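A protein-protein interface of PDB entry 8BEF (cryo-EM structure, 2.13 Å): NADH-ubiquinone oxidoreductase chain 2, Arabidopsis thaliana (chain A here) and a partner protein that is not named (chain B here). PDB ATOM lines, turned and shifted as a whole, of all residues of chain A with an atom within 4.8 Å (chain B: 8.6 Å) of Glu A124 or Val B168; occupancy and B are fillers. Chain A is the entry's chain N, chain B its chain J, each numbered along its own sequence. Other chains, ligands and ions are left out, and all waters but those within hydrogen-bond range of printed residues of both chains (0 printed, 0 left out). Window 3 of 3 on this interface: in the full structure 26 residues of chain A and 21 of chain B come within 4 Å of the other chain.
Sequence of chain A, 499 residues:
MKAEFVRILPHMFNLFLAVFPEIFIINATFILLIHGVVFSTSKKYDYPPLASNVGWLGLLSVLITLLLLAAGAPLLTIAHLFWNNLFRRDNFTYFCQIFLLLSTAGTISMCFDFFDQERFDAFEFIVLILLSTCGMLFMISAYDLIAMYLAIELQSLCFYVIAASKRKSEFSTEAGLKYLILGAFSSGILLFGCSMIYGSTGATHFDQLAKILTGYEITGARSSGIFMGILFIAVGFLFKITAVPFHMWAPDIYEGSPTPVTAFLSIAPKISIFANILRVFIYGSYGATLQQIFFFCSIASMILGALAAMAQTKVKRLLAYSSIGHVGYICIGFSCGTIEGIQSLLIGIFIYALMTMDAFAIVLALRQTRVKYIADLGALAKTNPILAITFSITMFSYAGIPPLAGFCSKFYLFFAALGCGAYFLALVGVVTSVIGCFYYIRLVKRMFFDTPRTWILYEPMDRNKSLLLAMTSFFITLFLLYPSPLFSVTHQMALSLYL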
ATOM      1  N   ALA A 122      10.001 -15.431   4.079  1.00  0.00           N
ATOM      2  CA  ALA A 122      10.309 -15.956   5.408  1.00  0.00           C
ATOM      3  C   ALA A 122      10.478 -17.470   5.352  1.00  0.00           C
ATOM      4  O   ALA A 122       9.504 -18.205   5.171  1.00  0.00           O
ATOM      5  CB  ALA A 122       9.215 -15.567   6.397  1.00  0.00           C
ATOM      6  N   PHE A 123      11.718 -17.941   5.506  1.00  0.00           N
ATOM      7  CA  PHE A 123      11.958 -19.377   5.606  1.00  0.00           C
ATOM      8  C   PHE A 123      11.472 -19.948   6.931  1.00  0.00           C
ATOM      9  O   PHE A 123      11.270 -21.162   7.031  1.00  0.00           O
ATOM     10  CB  PHE A 123      13.447 -19.684   5.436  1.00  0.00           C
ATOM     11  CG  PHE A 123      14.275 -19.336   6.639  1.00  0.00           C
ATOM     12  CD1 PHE A 123      14.494 -20.265   7.645  1.00  0.00           C
ATOM     13  CD2 PHE A 123      14.830 -18.075   6.766  1.00  0.00           C
ATOM     14  CE1 PHE A 123      15.247 -19.942   8.752  1.00  0.00           C
ATOM     15  CE2 PHE A 123      15.585 -17.748   7.872  1.00  0.00           C
ATOM     16  CZ  PHE A 123      15.793 -18.678   8.867  1.00  0.00           C
ATOM     17  N   GLU A 124      11.309 -19.104   7.953  1.00  0.00           N
ATOM     18  CA  GLU A 124      10.847 -19.581   9.253  1.00  0.00           C
ATOM     19  C   GLU A 124       9.475 -20.232   9.151  1.00  0.00           C
ATOM     20  O   GLU A 124       9.116 -21.060   9.992  1.00  0.00           O
ATOM     21  CB  GLU A 124      10.819 -18.424  10.253  1.00  0.00           C
ATOM     22  CG  GLU A 124      12.200 -17.922  10.661  1.00  0.00           C
ATOM     23  CD  GLU A 124      12.714 -16.792   9.777  1.00  0.00           C
ATOM     24  OE1 GLU A 124      12.292 -16.698   8.607  1.00  0.00           O
ATOM     25  OE2 GLU A 124      13.550 -16.001  10.258  1.00  0.00           O
ATOM     26  N   PHE A 125       8.699 -19.859   8.134  1.00  0.00           N
ATOM     27  CA  PHE A 125       7.425 -20.508   7.844  1.00  0.00           C
ATOM     28  C   PHE A 125       7.591 -22.022   7.709  1.00  0.00           C
ATOM     29  O   PHE A 125       6.857 -22.807   8.328  1.00  0.00           O
ATOM     30  CB  PHE A 125       6.871 -19.888   6.559  1.00  0.00           C
ATOM     31  CG  PHE A 125       5.557 -20.428   6.124  1.00  0.00           C
ATOM     32  CD1 PHE A 125       4.394 -20.053   6.770  1.00  0.00           C
ATOM     33  CD2 PHE A 125       5.476 -21.291   5.047  1.00  0.00           C
ATOM     34  CE1 PHE A 125       3.180 -20.543   6.356  1.00  0.00           C
ATOM     35  CE2 PHE A 125       4.258 -21.780   4.627  1.00  0.00           C
ATOM     36  CZ  PHE A 125       3.111 -21.410   5.286  1.00  0.00           C
ATOM     37  N   ILE A 126       8.579 -22.448   6.918  1.00  0.00           N
ATOM     38  CA  ILE A 126       8.832 -23.873   6.715  1.00  0.00           C
ATOM     39  C   ILE A 126       9.269 -24.533   8.019  1.00  0.00           C
ATOM     40  O   ILE A 126       8.841 -25.648   8.340  1.00  0.00           O
ATOM     41  CB  ILE A 126       9.880 -24.070   5.603  1.00  0.00           C
ATOM     42  CG1 ILE A 126       9.291 -23.745   4.227  1.00  0.00           C
ATOM     43  CG2 ILE A 126      10.391 -25.506   5.601  1.00  0.00           C
ATOM     44  CD1 ILE A 126       7.900 -24.294   3.991  1.00  0.00           C
ATOM     45  N   VAL A 127      10.140 -23.864   8.779  1.00  0.00           N
ATOM     46  CA  VAL A 127      10.610 -24.414  10.050  1.00  0.00           C
ATOM     47  C   VAL A 127       9.451 -24.620  11.013  1.00  0.00           C
ATOM     48  O   VAL A 127       9.374 -25.641  11.705  1.00  0.00           O
ATOM     49  CB  VAL A 127      11.698 -23.508  10.657  1.00  0.00           C
ATOM     50  CG1 VAL A 127      12.279 -24.146  11.907  1.00  0.00           C
ATOM     51  CG2 VAL A 127      12.804 -23.267   9.641  1.00  0.00           C
ATOM     52  N   LEU A 128       8.539 -23.651  11.085  1.00  0.00           N
ATOM     53  CA  LEU A 128       7.393 -23.781  11.975  1.00  0.00           C
ATOM     54  C   LEU A 128       6.471 -24.904  11.520  1.00  0.00           C
ATOM     55  O   LEU A 128       5.928 -25.638  12.353  1.00  0.00           O
ATOM     56  CB  LEU A 128       6.640 -22.455  12.064  1.00  0.00           C
ATOM     57  CG  LEU A 128       7.416 -21.293  12.696  1.00  0.00           C
ATOM     58  CD1 LEU A 128       6.853 -19.959  12.241  1.00  0.00           C
ATOM     59  CD2 LEU A 128       7.427 -21.372  14.213  1.00  0.00           C
ATOM     60  N   VAL A 161       1.534 -18.950  15.455  1.00  0.00           N
ATOM     61  CA  VAL A 161       2.542 -18.104  14.822  1.00  0.00           C
ATOM     62  C   VAL A 161       2.325 -18.024  13.313  1.00  0.00           C
ATOM     63  O   VAL A 161       2.389 -16.937  12.727  1.00  0.00           O
ATOM     64  CB  VAL A 161       3.960 -18.588  15.168  1.00  0.00           C
ATOM     65  CG1 VAL A 161       4.987 -17.796  14.376  1.00  0.00           C
ATOM     66  CG2 VAL A 161       4.210 -18.443  16.656  1.00  0.00           C
ATOM     67  N   ARG A 167       2.249 -10.253   8.946  1.00  0.00           N
ATOM     68  CA  ARG A 167       2.167  -9.467  10.171  1.00  0.00           C
ATOM     69  C   ARG A 167       1.790  -8.002   9.947  1.00  0.00           C
ATOM     70  O   ARG A 167       1.474  -7.316  10.923  1.00  0.00           O
ATOM     71  CB  ARG A 167       3.497  -9.568  10.924  1.00  0.00           C
ATOM     72  CG  ARG A 167       4.607  -8.785  10.278  1.00  0.00           C
ATOM     73  CD  ARG A 167       5.990  -9.214  10.718  1.00  0.00           C
ATOM     74  NE  ARG A 167       6.992  -8.273  10.230  1.00  0.00           N
ATOM     75  CZ  ARG A 167       8.162  -8.042  10.809  1.00  0.00           C
ATOM     76  NH1 ARG A 167       8.542  -8.704  11.892  1.00  0.00           N
ATOM     77  NH2 ARG A 167       8.970  -7.122  10.291  1.00  0.00           N
ATOM     78  N   VAL B 161       9.887 -22.688  19.781  1.00  0.00           N
ATOM     79  CA  VAL B 161       8.822 -22.091  18.980  1.00  0.00           C
ATOM     80  C   VAL B 161       8.518 -20.684  19.473  1.00  0.00           C
ATOM     81  O   VAL B 161       8.326 -19.761  18.674  1.00  0.00           O
ATOM     82  CB  VAL B 161       7.562 -22.978  18.997  1.00  0.00           C
ATOM     83  CG1 VAL B 161       6.384 -22.236  18.376  1.00  0.00           C
ATOM     84  CG2 VAL B 161       7.817 -24.275  18.259  1.00  0.00           C
ATOM     85  N   ALA B 162       8.456 -20.500  20.795  1.00  0.00           N
ATOM     86  CA  ALA B 162       8.188 -19.166  21.333  1.00  0.00           C
ATOM     87  C   ALA B 162       9.242 -18.162  20.875  1.00  0.00           C
ATOM     88  O   ALA B 162       8.911 -17.050  20.447  1.00  0.00           O
ATOM     89  CB  ALA B 162       8.118 -19.209  22.860  1.00  0.00           C
ATOM     90  N   MET B 163      10.519 -18.545  20.950  1.00  0.00           N
ATOM     91  CA  MET B 163      11.595 -17.640  20.539  1.00  0.00           C
ATOM     92  C   MET B 163      11.472 -17.268  19.063  1.00  0.00           C
ATOM     93  O   MET B 163      11.517 -16.081  18.692  1.00  0.00           O
ATOM     94  CB  MET B 163      12.954 -18.287  20.820  1.00  0.00           C
ATOM     95  CG  MET B 163      13.043 -18.927  22.192  1.00  0.00           C
ATOM     96  SD  MET B 163      14.491 -19.954  22.515  1.00  0.00           S
ATOM     97  CE  MET B 163      15.817 -18.782  22.334  1.00  0.00           C
ATOM     98  N   ILE B 164      11.294 -18.277  18.207  1.00  0.00           N
ATOM     99  CA  ILE B 164      11.199 -18.028  16.771  1.00  0.00           C
ATOM    100  C   ILE B 164      10.011 -17.126  16.466  1.00  0.00           C
ATOM    101  O   ILE B 164      10.124 -16.163  15.699  1.00  0.00           O
ATOM    102  CB  ILE B 164      11.108 -19.354  15.996  1.00  0.00           C
ATOM    103  CG1 ILE B 164      12.451 -20.085  16.015  1.00  0.00           C
ATOM    104  CG2 ILE B 164      10.647 -19.103  14.565  1.00  0.00           C
ATOM    105  CD1 ILE B 164      12.388 -21.479  15.429  1.00  0.00           C
ATOM    106  N   GLY B 165       8.852 -17.431  17.056  1.00  0.00           N
ATOM    107  CA  GLY B 165       7.663 -16.637  16.794  1.00  0.00           C
ATOM    108  C   GLY B 165       7.806 -15.199  17.250  1.00  0.00           C
ATOM    109  O   GLY B 165       7.414 -14.270  16.537  1.00  0.00           O
ATOM    110  N   ALA B 166       8.380 -14.996  18.440  1.00  0.00           N
ATOM    111  CA  ALA B 166       8.617 -13.642  18.923  1.00  0.00           C
ATOM    112  C   ALA B 166       9.471 -12.856  17.942  1.00  0.00           C
ATOM    113  O   ALA B 166       9.173 -11.693  17.646  1.00  0.00           O
ATOM    114  CB  ALA B 166       9.278 -13.677  20.299  1.00  0.00           C
ATOM    115  N   ILE B 167      10.533 -13.471  17.417  1.00  0.00           N
ATOM    116  CA  ILE B 167      11.360 -12.752  16.448  1.00  0.00           C
ATOM    117  C   ILE B 167      10.576 -12.469  15.167  1.00  0.00           C
ATOM    118  O   ILE B 167      10.497 -11.323  14.716  1.00  0.00           O
ATOM    119  CB  ILE B 167      12.660 -13.520  16.154  1.00  0.00           C
ATOM    120  CG1 ILE B 167      13.572 -13.533  17.383  1.00  0.00           C
ATOM    121  CG2 ILE B 167      13.369 -12.895  14.958  1.00  0.00           C
ATOM    122  CD1 ILE B 167      13.716 -12.194  18.065  1.00  0.00           C
ATOM    123  N   VAL B 168       9.962 -13.499  14.580  1.00  0.00           N
ATOM    124  CA  VAL B 168       9.387 -13.341  13.243  1.00  0.00           C
ATOM    125  C   VAL B 168       8.222 -12.360  13.249  1.00  0.00           C
ATOM    126  O   VAL B 168       7.990 -11.662  12.257  1.00  0.00           O
ATOM    127  CB  VAL B 168       8.959 -14.698  12.646  1.00  0.00           C
ATOM    128  CG1 VAL B 168      10.148 -15.634  12.531  1.00  0.00           C
ATOM    129  CG2 VAL B 168       7.841 -15.325  13.463  1.00  0.00           C
ATOM    130  N   LEU B 169       7.471 -12.277  14.348  1.00  0.00           N
ATOM    131  CA  LEU B 169       6.288 -11.429  14.323  1.00  0.00           C
ATOM    132  C   LEU B 169       6.593  -9.966  14.635  1.00  0.00           C
ATOM    133  O   LEU B 169       5.920  -9.081  14.102  1.00  0.00           O
ATOM    134  CB  LEU B 169       5.233 -11.977  15.283  1.00  0.00           C
ATOM    135  CG  LEU B 169       4.746 -13.378  14.895  1.00  0.00           C
ATOM    136  CD1 LEU B 169       4.226 -14.153  16.093  1.00  0.00           C
ATOM    137  CD2 LEU B 169       3.704 -13.303  13.787  1.00  0.00           C
ATOM    138  N   THR B 170       7.602  -9.677  15.459  1.00  0.00           N
ATOM    139  CA  THR B 170       7.794  -8.318  15.952  1.00  0.00           C
ATOM    140  C   THR B 170       9.082  -7.635  15.508  1.00  0.00           C
ATOM    141  O   THR B 170       9.156  -6.407  15.602  1.00  0.00           O
ATOM    142  CB  THR B 170       7.743  -8.288  17.490  1.00  0.00           C
ATOM    143  OG1 THR B 170       8.824  -9.057  18.025  1.00  0.00           O
ATOM    144  CG2 THR B 170       6.419  -8.855  17.995  1.00  0.00           C
ATOM    145  N   MET B 171      10.081  -8.370  15.027  1.00  0.00           N
ATOM    146  CA  MET B 171      11.390  -7.779  14.763  1.00  0.00           C
ATOM    147  C   MET B 171      11.334  -6.761  13.628  1.00  0.00           C
ATOM    148  O   MET B 171      10.828  -7.047  12.540  1.00  0.00           O
ATOM    149  CB  MET B 171      12.405  -8.872  14.429  1.00  0.00           C
ATOM    150  CG  MET B 171      13.825  -8.378  14.188  1.00  0.00           C
ATOM    151  SD  MET B 171      14.292  -6.966  15.207  1.00  0.00           S
ATOM    152  CE  MET B 171      15.410  -7.756  16.357  1.00  0.00           C
ATOM    153  N   HIS B 172      11.870  -5.570  13.893  1.00  0.00           N
ATOM    154  CA  HIS B 172      12.137  -4.545  12.883  1.00  0.00           C
ATOM    155  C   HIS B 172      13.571  -4.089  13.135  1.00  0.00           C
ATOM    156  O   HIS B 172      13.812  -3.237  13.993  1.00  0.00           O
ATOM    157  CB  HIS B 172      11.148  -3.384  12.970  1.00  0.00           C
ATOM    158  CG  HIS B 172       9.784  -3.705  12.446  1.00  0.00           C
ATOM    159  ND1 HIS B 172       8.874  -4.462  13.151  1.00  0.00           N
ATOM    160  CD2 HIS B 172       9.173  -3.367  11.286  1.00  0.00           C
ATOM    161  CE1 HIS B 172       7.763  -4.579  12.447  1.00  0.00           C
ATOM    162  NE2 HIS B 172       7.919  -3.926  11.311  1.00  0.00           N
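O of Leu B169 sits close to NH1 of Arg A167 (3.4 Å).
NH1 of Arg A167 sits at hydrogen-bond distance from O of Val B168, 3.0 Å away.
O of Met B171 is in hydrogen-bond range of NH1 of Arg A167, 2.9 Å away.
OG1 of Thr B170 lies within hydrogen-bond range of O of Ala B166, at 2.7 Å.
The backbone carbonyl oxygen (O) of Thr B170 sits at hydrogen-bond distance from a ring nitrogen (ND1) of His B172 (3.1 Å).
Val B168 touches Glu A124 (CG1 to CG, 3.6 Å).
Leu A128 touches Ile B164.
Gly B165 touches Val A161 (CA to CG1, 3.8 Å).
Val B168 touches Val A161 (CG2 to CG1, 3.9 Å).
C of Thr B170 touches NH1 of Arg A167 (3.8 Å).
NE2 of His B172 touches NH2 of Arg A167 (3.5 Å).
Of the 12 printed residues of chain B, 7 touch a printed residue of chain A.
Of the 9 printed residues of chain A, 4 touch a printed residue of chain B.
Hydrophobic or aromatic side chains of chain A within 4 Å of the printed part of chain B: Leu A128 and Val A161.
Along chain A the printed residues that touch a printed residue of chain B span positions 124 to 167.
Among the printed residues, no Asp or Glu carboxylate lies within 4 Å of a Lys or Arg side-chain nitrogen of the other chain.
Val B168 touches three residues of chain A.
No residue of chain B comes within 4 Å of Phe A123.
Of the printed residues of chain A, Leu B169 touches Arg A167.
Printed residues of chain A within 4 Å of Met B171: Arg A167 (2.9 Å).
Printed residues of chain A within 4 Å of Gly B165: Val A161.
Printed residues of chain B within 4 Å of Leu A128: Ile B164.
Val B161 touches none of the printed residues of chain A.
Ala A122 touches none of the printed residues of chain B.
The nearest residue of chain B that does not touch Glu A124 is Ile B164 (4.4 Å).
The nearest printed residue of chain A that does not touch His B172 is Glu A124 (11.2 Å).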
